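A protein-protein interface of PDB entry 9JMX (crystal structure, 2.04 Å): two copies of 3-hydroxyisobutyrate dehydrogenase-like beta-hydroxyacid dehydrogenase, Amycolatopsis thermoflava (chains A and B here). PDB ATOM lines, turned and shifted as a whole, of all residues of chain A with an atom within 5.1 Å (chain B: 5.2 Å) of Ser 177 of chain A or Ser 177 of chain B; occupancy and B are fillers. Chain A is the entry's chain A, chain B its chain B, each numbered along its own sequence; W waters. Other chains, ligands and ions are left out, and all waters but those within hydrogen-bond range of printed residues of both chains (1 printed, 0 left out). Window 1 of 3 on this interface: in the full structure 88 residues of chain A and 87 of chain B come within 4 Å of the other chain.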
ATOM      1  N   THR A 172     -29.608  15.444  12.187  1.00  0.00           N
ATOM      2  CA  THR A 172     -28.962  14.986  13.436  1.00  0.00           C
ATOM      3  C   THR A 172     -27.447  15.137  13.287  1.00  0.00           C
ATOM      4  O   THR A 172     -26.790  15.528  14.257  1.00  0.00           O
ATOM      5  CB  THR A 172     -29.245  13.530  13.816  1.00  0.00           C
ATOM      6  OG1 THR A 172     -30.604  13.227  13.501  1.00  0.00           O
ATOM      7  CG2 THR A 172     -28.965  13.317  15.286  1.00  0.00           C
ATOM      8  N   VAL A 173     -26.927  14.793  12.108  1.00  0.00           N
ATOM      9  CA  VAL A 173     -25.482  14.900  11.795  1.00  0.00           C
ATOM     10  C   VAL A 173     -25.132  16.382  11.768  1.00  0.00           C
ATOM     11  O   VAL A 173     -24.240  16.807  12.523  1.00  0.00           O
ATOM     12  CB  VAL A 173     -25.121  14.195  10.475  1.00  0.00           C
ATOM     13  CG1 VAL A 173     -23.655  14.402  10.133  1.00  0.00           C
ATOM     14  CG2 VAL A 173     -25.456  12.721  10.568  1.00  0.00           C
ATOM     15  N   PHE A 174     -25.884  17.144  10.998  1.00  0.00           N
ATOM     16  CA  PHE A 174     -25.544  18.552  10.685  1.00  0.00           C
ATOM     17  C   PHE A 174     -25.667  19.398  11.952  1.00  0.00           C
ATOM     18  O   PHE A 174     -24.654  20.031  12.300  1.00  0.00           O
ATOM     19  CB  PHE A 174     -26.392  19.027   9.519  1.00  0.00           C
ATOM     20  CG  PHE A 174     -26.187  20.473   9.183  1.00  0.00           C
ATOM     21  CD1 PHE A 174     -25.083  20.872   8.450  1.00  0.00           C
ATOM     22  CD2 PHE A 174     -27.086  21.426   9.622  1.00  0.00           C
ATOM     23  CE1 PHE A 174     -24.904  22.200   8.131  1.00  0.00           C
ATOM     24  CE2 PHE A 174     -26.886  22.759   9.327  1.00  0.00           C
ATOM     25  CZ  PHE A 174     -25.804  23.138   8.567  1.00  0.00           C
ATOM     26  N   LEU A 175     -26.826  19.399  12.636  1.00  0.00           N
ATOM     27  CA  LEU A 175     -27.060  20.290  13.802  1.00  0.00           C
ATOM     28  C   LEU A 175     -26.171  19.863  14.977  1.00  0.00           C
ATOM     29  O   LEU A 175     -25.687  20.748  15.680  1.00  0.00           O
ATOM     30  CB  LEU A 175     -28.535  20.268  14.206  1.00  0.00           C
ATOM     31  CG  LEU A 175     -29.523  20.920  13.227  1.00  0.00           C
ATOM     32  CD1 LEU A 175     -30.948  20.772  13.741  1.00  0.00           C
ATOM     33  CD2 LEU A 175     -29.193  22.383  13.005  1.00  0.00           C
ATOM     34  N   THR A 176     -25.981  18.560  15.207  1.00  0.00           N
ATOM     35  CA  THR A 176     -25.161  18.053  16.335  1.00  0.00           C
ATOM     36  C   THR A 176     -23.695  18.463  16.102  1.00  0.00           C
ATOM     37  O   THR A 176     -23.046  18.888  17.061  1.00  0.00           O
ATOM     38  CB  THR A 176     -25.340  16.548  16.559  1.00  0.00           C
ATOM     39  OG1 THR A 176     -26.734  16.241  16.625  1.00  0.00           O
ATOM     40  CG2 THR A 176     -24.658  16.094  17.825  1.00  0.00           C
ATOM     41  N   SER A 177     -23.204  18.358  14.868  1.00  0.00           N
ATOM     42  CA  SER A 177     -21.850  18.791  14.467  1.00  0.00           C
ATOM     43  C   SER A 177     -21.712  20.286  14.723  1.00  0.00           C
ATOM     44  O   SER A 177     -20.744  20.648  15.399  1.00  0.00           O
ATOM     45  CB  SER A 177     -21.515  18.422  13.024  1.00  0.00           C
ATOM     46  OG  SER A 177     -21.681  17.033  12.857  1.00  0.00           O
ATOM     47  N   LEU A 178     -22.654  21.102  14.248  1.00  0.00           N
ATOM     48  CA  LEU A 178     -22.641  22.559  14.521  1.00  0.00           C
ATOM     49  C   LEU A 178     -22.548  22.777  16.029  1.00  0.00           C
ATOM     50  O   LEU A 178     -21.703  23.609  16.415  1.00  0.00           O
ATOM     51  CB  LEU A 178     -23.857  23.278  13.927  1.00  0.00           C
ATOM     52  CG  LEU A 178     -23.873  23.326  12.399  1.00  0.00           C
ATOM     53  CD1 LEU A 178     -24.995  24.220  11.886  1.00  0.00           C
ATOM     54  CD2 LEU A 178     -22.533  23.781  11.859  1.00  0.00           C
ATOM     55  N   SER A 179     -23.344  22.072  16.849  1.00  0.00           N
ATOM     56  CA  SER A 179     -23.291  22.260  18.321  1.00  0.00           C
ATOM     57  C   SER A 179     -21.895  21.892  18.843  1.00  0.00           C
ATOM     58  O   SER A 179     -21.448  22.595  19.766  1.00  0.00           O
ATOM     59  CB  SER A 179     -24.395  21.544  19.067  1.00  0.00           C
ATOM     60  OG  SER A 179     -25.644  22.203  18.848  1.00  0.00           O
ATOM     61  N   ALA A 180     -21.266  20.838  18.296  1.00  0.00           N
ATOM     62  CA  ALA A 180     -19.917  20.367  18.687  1.00  0.00           C
ATOM     63  C   ALA A 180     -18.868  21.436  18.341  1.00  0.00           C
ATOM     64  O   ALA A 180     -17.931  21.618  19.136  1.00  0.00           O
ATOM     65  CB  ALA A 180     -19.589  19.057  18.024  1.00  0.00           C
ATOM     66  N   TYR A 181     -19.009  22.123  17.212  1.00  0.00           N
ATOM     67  CA  TYR A 181     -18.169  23.305  16.867  1.00  0.00           C
ATOM     68  C   TYR A 181     -18.288  24.367  17.977  1.00  0.00           C
ATOM     69  O   TYR A 181     -17.253  24.801  18.476  1.00  0.00           O
ATOM     70  CB  TYR A 181     -18.533  23.880  15.492  1.00  0.00           C
ATOM     71  CG  TYR A 181     -18.179  23.006  14.316  1.00  0.00           C
ATOM     72  CD1 TYR A 181     -17.154  22.072  14.397  1.00  0.00           C
ATOM     73  CD2 TYR A 181     -18.859  23.125  13.115  1.00  0.00           C
ATOM     74  CE1 TYR A 181     -16.807  21.287  13.314  1.00  0.00           C
ATOM     75  CE2 TYR A 181     -18.532  22.333  12.027  1.00  0.00           C
ATOM     76  CZ  TYR A 181     -17.500  21.419  12.130  1.00  0.00           C
ATOM     77  OH  TYR A 181     -17.151  20.646  11.069  1.00  0.00           O
ATOM     78  N   ALA A 209     -13.533  12.252  10.975  1.00  0.00           N
ATOM     79  CA  ALA A 209     -14.788  11.664  11.506  1.00  0.00           C
ATOM     80  C   ALA A 209     -15.554  10.980  10.372  1.00  0.00           C
ATOM     81  O   ALA A 209     -15.974   9.817  10.582  1.00  0.00           O
ATOM     82  CB  ALA A 209     -15.661  12.708  12.163  1.00  0.00           C
ATOM     83  N   THR B 172     -13.949  16.880  21.133  1.00  0.00           N
ATOM     84  CA  THR B 172     -15.350  17.338  21.321  1.00  0.00           C
ATOM     85  C   THR B 172     -16.039  17.225  19.964  1.00  0.00           C
ATOM     86  O   THR B 172     -17.073  16.591  19.862  1.00  0.00           O
ATOM     87  CB  THR B 172     -15.426  18.781  21.847  1.00  0.00           C
ATOM     88  OG1 THR B 172     -14.765  18.820  23.108  1.00  0.00           O
ATOM     89  CG2 THR B 172     -16.850  19.254  22.000  1.00  0.00           C
ATOM     90  N   VAL B 173     -15.394  17.772  18.946  1.00  0.00           N
ATOM     91  CA  VAL B 173     -15.890  17.726  17.560  1.00  0.00           C
ATOM     92  C   VAL B 173     -15.989  16.273  17.100  1.00  0.00           C
ATOM     93  O   VAL B 173     -17.037  15.911  16.512  1.00  0.00           O
ATOM     94  CB  VAL B 173     -15.016  18.552  16.617  1.00  0.00           C
ATOM     95  CG1 VAL B 173     -15.572  18.461  15.204  1.00  0.00           C
ATOM     96  CG2 VAL B 173     -14.926  19.993  17.089  1.00  0.00           C
ATOM     97  N   PHE B 174     -14.931  15.506  17.322  1.00  0.00           N
ATOM     98  CA  PHE B 174     -14.724  14.156  16.736  1.00  0.00           C
ATOM     99  C   PHE B 174     -15.666  13.142  17.396  1.00  0.00           C
ATOM    100  O   PHE B 174     -16.462  12.540  16.710  1.00  0.00           O
ATOM    101  CB  PHE B 174     -13.258  13.733  16.869  1.00  0.00           C
ATOM    102  CG  PHE B 174     -12.994  12.365  16.322  1.00  0.00           C
ATOM    103  CD1 PHE B 174     -12.969  12.154  14.951  1.00  0.00           C
ATOM    104  CD2 PHE B 174     -12.871  11.274  17.172  1.00  0.00           C
ATOM    105  CE1 PHE B 174     -12.758  10.884  14.436  1.00  0.00           C
ATOM    106  CE2 PHE B 174     -12.663   9.998  16.658  1.00  0.00           C
ATOM    107  CZ  PHE B 174     -12.634   9.807  15.294  1.00  0.00           C
ATOM    108  N   LEU B 175     -15.615  13.004  18.711  1.00  0.00           N
ATOM    109  CA  LEU B 175     -16.465  12.023  19.420  1.00  0.00           C
ATOM    110  C   LEU B 175     -17.946  12.412  19.261  1.00  0.00           C
ATOM    111  O   LEU B 175     -18.787  11.499  19.089  1.00  0.00           O
ATOM    112  CB  LEU B 175     -16.054  11.946  20.890  1.00  0.00           C
ATOM    113  CG  LEU B 175     -14.675  11.353  21.181  1.00  0.00           C
ATOM    114  CD1 LEU B 175     -14.455  11.272  22.689  1.00  0.00           C
ATOM    115  CD2 LEU B 175     -14.508   9.976  20.545  1.00  0.00           C
ATOM    116  N   THR B 176     -18.286  13.696  19.298  1.00  0.00           N
ATOM    117  CA  THR B 176     -19.710  14.109  19.168  1.00  0.00           C
ATOM    118  C   THR B 176     -20.167  13.815  17.737  1.00  0.00           C
ATOM    119  O   THR B 176     -21.291  13.347  17.575  1.00  0.00           O
ATOM    120  CB  THR B 176     -19.979  15.562  19.576  1.00  0.00           C
ATOM    121  OG1 THR B 176     -19.400  15.747  20.868  1.00  0.00           O
ATOM    122  CG2 THR B 176     -21.464  15.856  19.609  1.00  0.00           C
ATOM    123  N   SER B 177     -19.318  14.033  16.735  1.00  0.00           N
ATOM    124  CA  SER B 177     -19.669  13.724  15.335  1.00  0.00           C
ATOM    125  C   SER B 177     -19.931  12.220  15.193  1.00  0.00           C
ATOM    126  O   SER B 177     -20.944  11.843  14.559  1.00  0.00           O
ATOM    127  CB  SER B 177     -18.608  14.212  14.389  1.00  0.00           C
ATOM    128  OG  SER B 177     -18.508  15.625  14.466  1.00  0.00           O
ATOM    129  N   LEU B 178     -19.094  11.375  15.784  1.00  0.00           N
ATOM    130  CA  LEU B 178     -19.296   9.900  15.717  1.00  0.00           C
ATOM    131  C   LEU B 178     -20.639   9.521  16.373  1.00  0.00           C
ATOM    132  O   LEU B 178     -21.342   8.699  15.781  1.00  0.00           O
ATOM    133  CB  LEU B 178     -18.135   9.162  16.395  1.00  0.00           C
ATOM    134  CG  LEU B 178     -16.766   9.270  15.711  1.00  0.00           C
ATOM    135  CD1 LEU B 178     -15.752   8.344  16.388  1.00  0.00           C
ATOM    136  CD2 LEU B 178     -16.861   8.991  14.217  1.00  0.00           C
ATOM    137  N   SER B 179     -20.978  10.076  17.549  1.00  0.00           N
ATOM    138  CA  SER B 179     -22.261   9.779  18.254  1.00  0.00           C
ATOM    139  C   SER B 179     -23.433  10.234  17.383  1.00  0.00           C
ATOM    140  O   SER B 179     -24.420   9.520  17.295  1.00  0.00           O
ATOM    141  CB  SER B 179     -22.333  10.394  19.615  1.00  0.00           C
ATOM    142  OG  SER B 179     -21.454   9.737  20.491  1.00  0.00           O
ATOM    143  N   ALA B 180     -23.269  11.344  16.680  1.00  0.00           N
ATOM    144  CA  ALA B 180     -24.294  11.902  15.780  1.00  0.00           C
ATOM    145  C   ALA B 180     -24.527  10.939  14.611  1.00  0.00           C
ATOM    146  O   ALA B 180     -25.679  10.863  14.132  1.00  0.00           O
ATOM    147  CB  ALA B 180     -23.862  13.261  15.291  1.00  0.00           C
ATOM    148  N   TYR B 181     -23.461  10.287  14.126  1.00  0.00           N
ATOM    149  CA  TYR B 181     -23.551   9.288  13.038  1.00  0.00           C
ATOM    150  C   TYR B 181     -24.352   8.093  13.563  1.00  0.00           C
ATOM    151  O   TYR B 181     -25.262   7.669  12.854  1.00  0.00           O
ATOM    152  CB  TYR B 181     -22.181   8.848  12.511  1.00  0.00           C
ATOM    153  CG  TYR B 181     -21.363   9.865  11.757  1.00  0.00           C
ATOM    154  CD1 TYR B 181     -21.924  10.818  10.925  1.00  0.00           C
ATOM    155  CD2 TYR B 181     -19.983   9.824  11.839  1.00  0.00           C
ATOM    156  CE1 TYR B 181     -21.146  11.712  10.208  1.00  0.00           C
ATOM    157  CE2 TYR B 181     -19.183  10.706  11.133  1.00  0.00           C
ATOM    158  CZ  TYR B 181     -19.762  11.667  10.332  1.00  0.00           C
ATOM    159  OH  TYR B 181     -18.934  12.516   9.653  1.00  0.00           O
ATOM    160  N   SER B 206     -21.687  16.520   6.527  1.00  0.00           N
ATOM    161  CA  SER B 206     -20.495  16.789   7.376  1.00  0.00           C
ATOM    162  C   SER B 206     -19.635  17.864   6.699  1.00  0.00           C
ATOM    163  O   SER B 206     -19.196  18.831   7.368  1.00  0.00           O
ATOM    164  CB  SER B 206     -19.720  15.550   7.619  1.00  0.00           C
ATOM    165  OG  SER B 206     -20.345  14.765   8.619  1.00  0.00           O
ATOM    166  N   ALA B 209     -21.556  21.166   7.118  1.00  0.00           N
ATOM    167  CA  ALA B 209     -21.326  21.687   8.481  1.00  0.00           C
ATOM    168  C   ALA B 209     -19.974  22.398   8.548  1.00  0.00           C
ATOM    169  O   ALA B 209     -19.922  23.506   9.103  1.00  0.00           O
ATOM    170  CB  ALA B 209     -21.361  20.569   9.475  1.00  0.00           C
HETATM  171  O   HOH W   1     -19.987  16.261  11.000  1.00  0.00           O
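The backbone carbonyl oxygen (O) of Thr 172 of chain A is in hydrogen-bond range of the side-chain hydroxyl (OG1) of Thr 176 of chain A (2.5 Å). OG of Ser 177 of chain A sits at hydrogen-bond distance from O of Val 173 of chain A (2.6 Å). The side-chain hydroxyl of Thr 176 of chain B is in hydrogen-bond range of the backbone carbonyl oxygen of Thr 172 of chain B (2.7 Å). OG of Ser 177 of chain B lies within hydrogen-bond range of O of Val 173 of chain B (2.5 Å). The side-chain hydroxyl (OH) of Tyr 181 of chain B is in hydrogen-bond range of the side-chain hydroxyl (OG) of Ser 206 of chain B (2.8 Å).
CB of Ala 180 of chain B touches O of Thr 172 of chain A, 3.8 Å away. Thr 176 of chain B touches Thr 176 of chain A. CB of Thr 176 of chain A touches CB of Ala 180 of chain B (3.8 Å). Ser 177 of chain B touches Ser 177 of chain A. Leu 178 of chain A touches Ala 209 of chain B (CD2 to O, 3.8 Å). Val 173 of chain B touches Ala 180 of chain A (CA to CB, 3.96 Å). Ala 180 of chain A touches Thr 176 of chain B. CB of Ala 209 of chain A touches CB of Ser 177 of chain B (3.99 Å). Leu 178 of chain B touches Ala 209 of chain A. O of Ala 209 of chain A touches CE2 of Tyr 181 of chain B (3.4 Å).
Ser 177 of chain A touches just one residue of chain B: Ser 177 (3.8 Å). Of the printed residues of chain A, Ser 177 of chain B touches Ser 177 and Ala 209. Of the printed residues of chain B, Phe 174 of chain A touches Ala 209. Of the printed residues of chain A, Ala 180 of chain B touches Thr 172 and Thr 176. Of the printed residues of chain A, Thr 176 of chain B touches Thr 176 and Ala 180. Printed residues of chain B within 4 Å of Leu 178 of chain A: Ala 209 (3.8 Å). Of the printed residues of chain B, Ala 180 of chain A touches Thr 172, Val 173 and Thr 176. The nearest residue of chain B that does not touch Ser 177 of chain A is Ala 209 of chain B (4.2 Å). The nearest printed residue of chain A that does not touch Ser 177 of chain B is Ala 180 of chain A (5.1 Å).
Of the 12 printed residues of chain B, 10 touch a printed residue of chain A. Hydrophobic or aromatic side chains of chain A within 4 Å of the printed part of chain B: Val 173, Phe 174, Leu 178, Ala 180, Tyr 181 and Ala 209.
Phe 174 of chain A touches Ala 209 of chain B, and with the chains exchanged Ala 209 of chain A touches Phe 174 of chain B. Thr 176 of chain A touches Ala 180 of chain B, and with the chains exchanged Ala 180 of chain A touches Thr 176 of chain B. Ser 177 of chain A touches its own counterpart, Ser 177 of chain B. Tyr 181 of chain A touches Ala 209 of chain B, and with the chains exchanged Ala 209 of chain A touches Tyr 181 of chain B.
Water W1 lies within hydrogen-bond range of OG of Ser 177 of chain A (2.6 Å) and OG of Ser 206 of chain B (2.8 Å).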
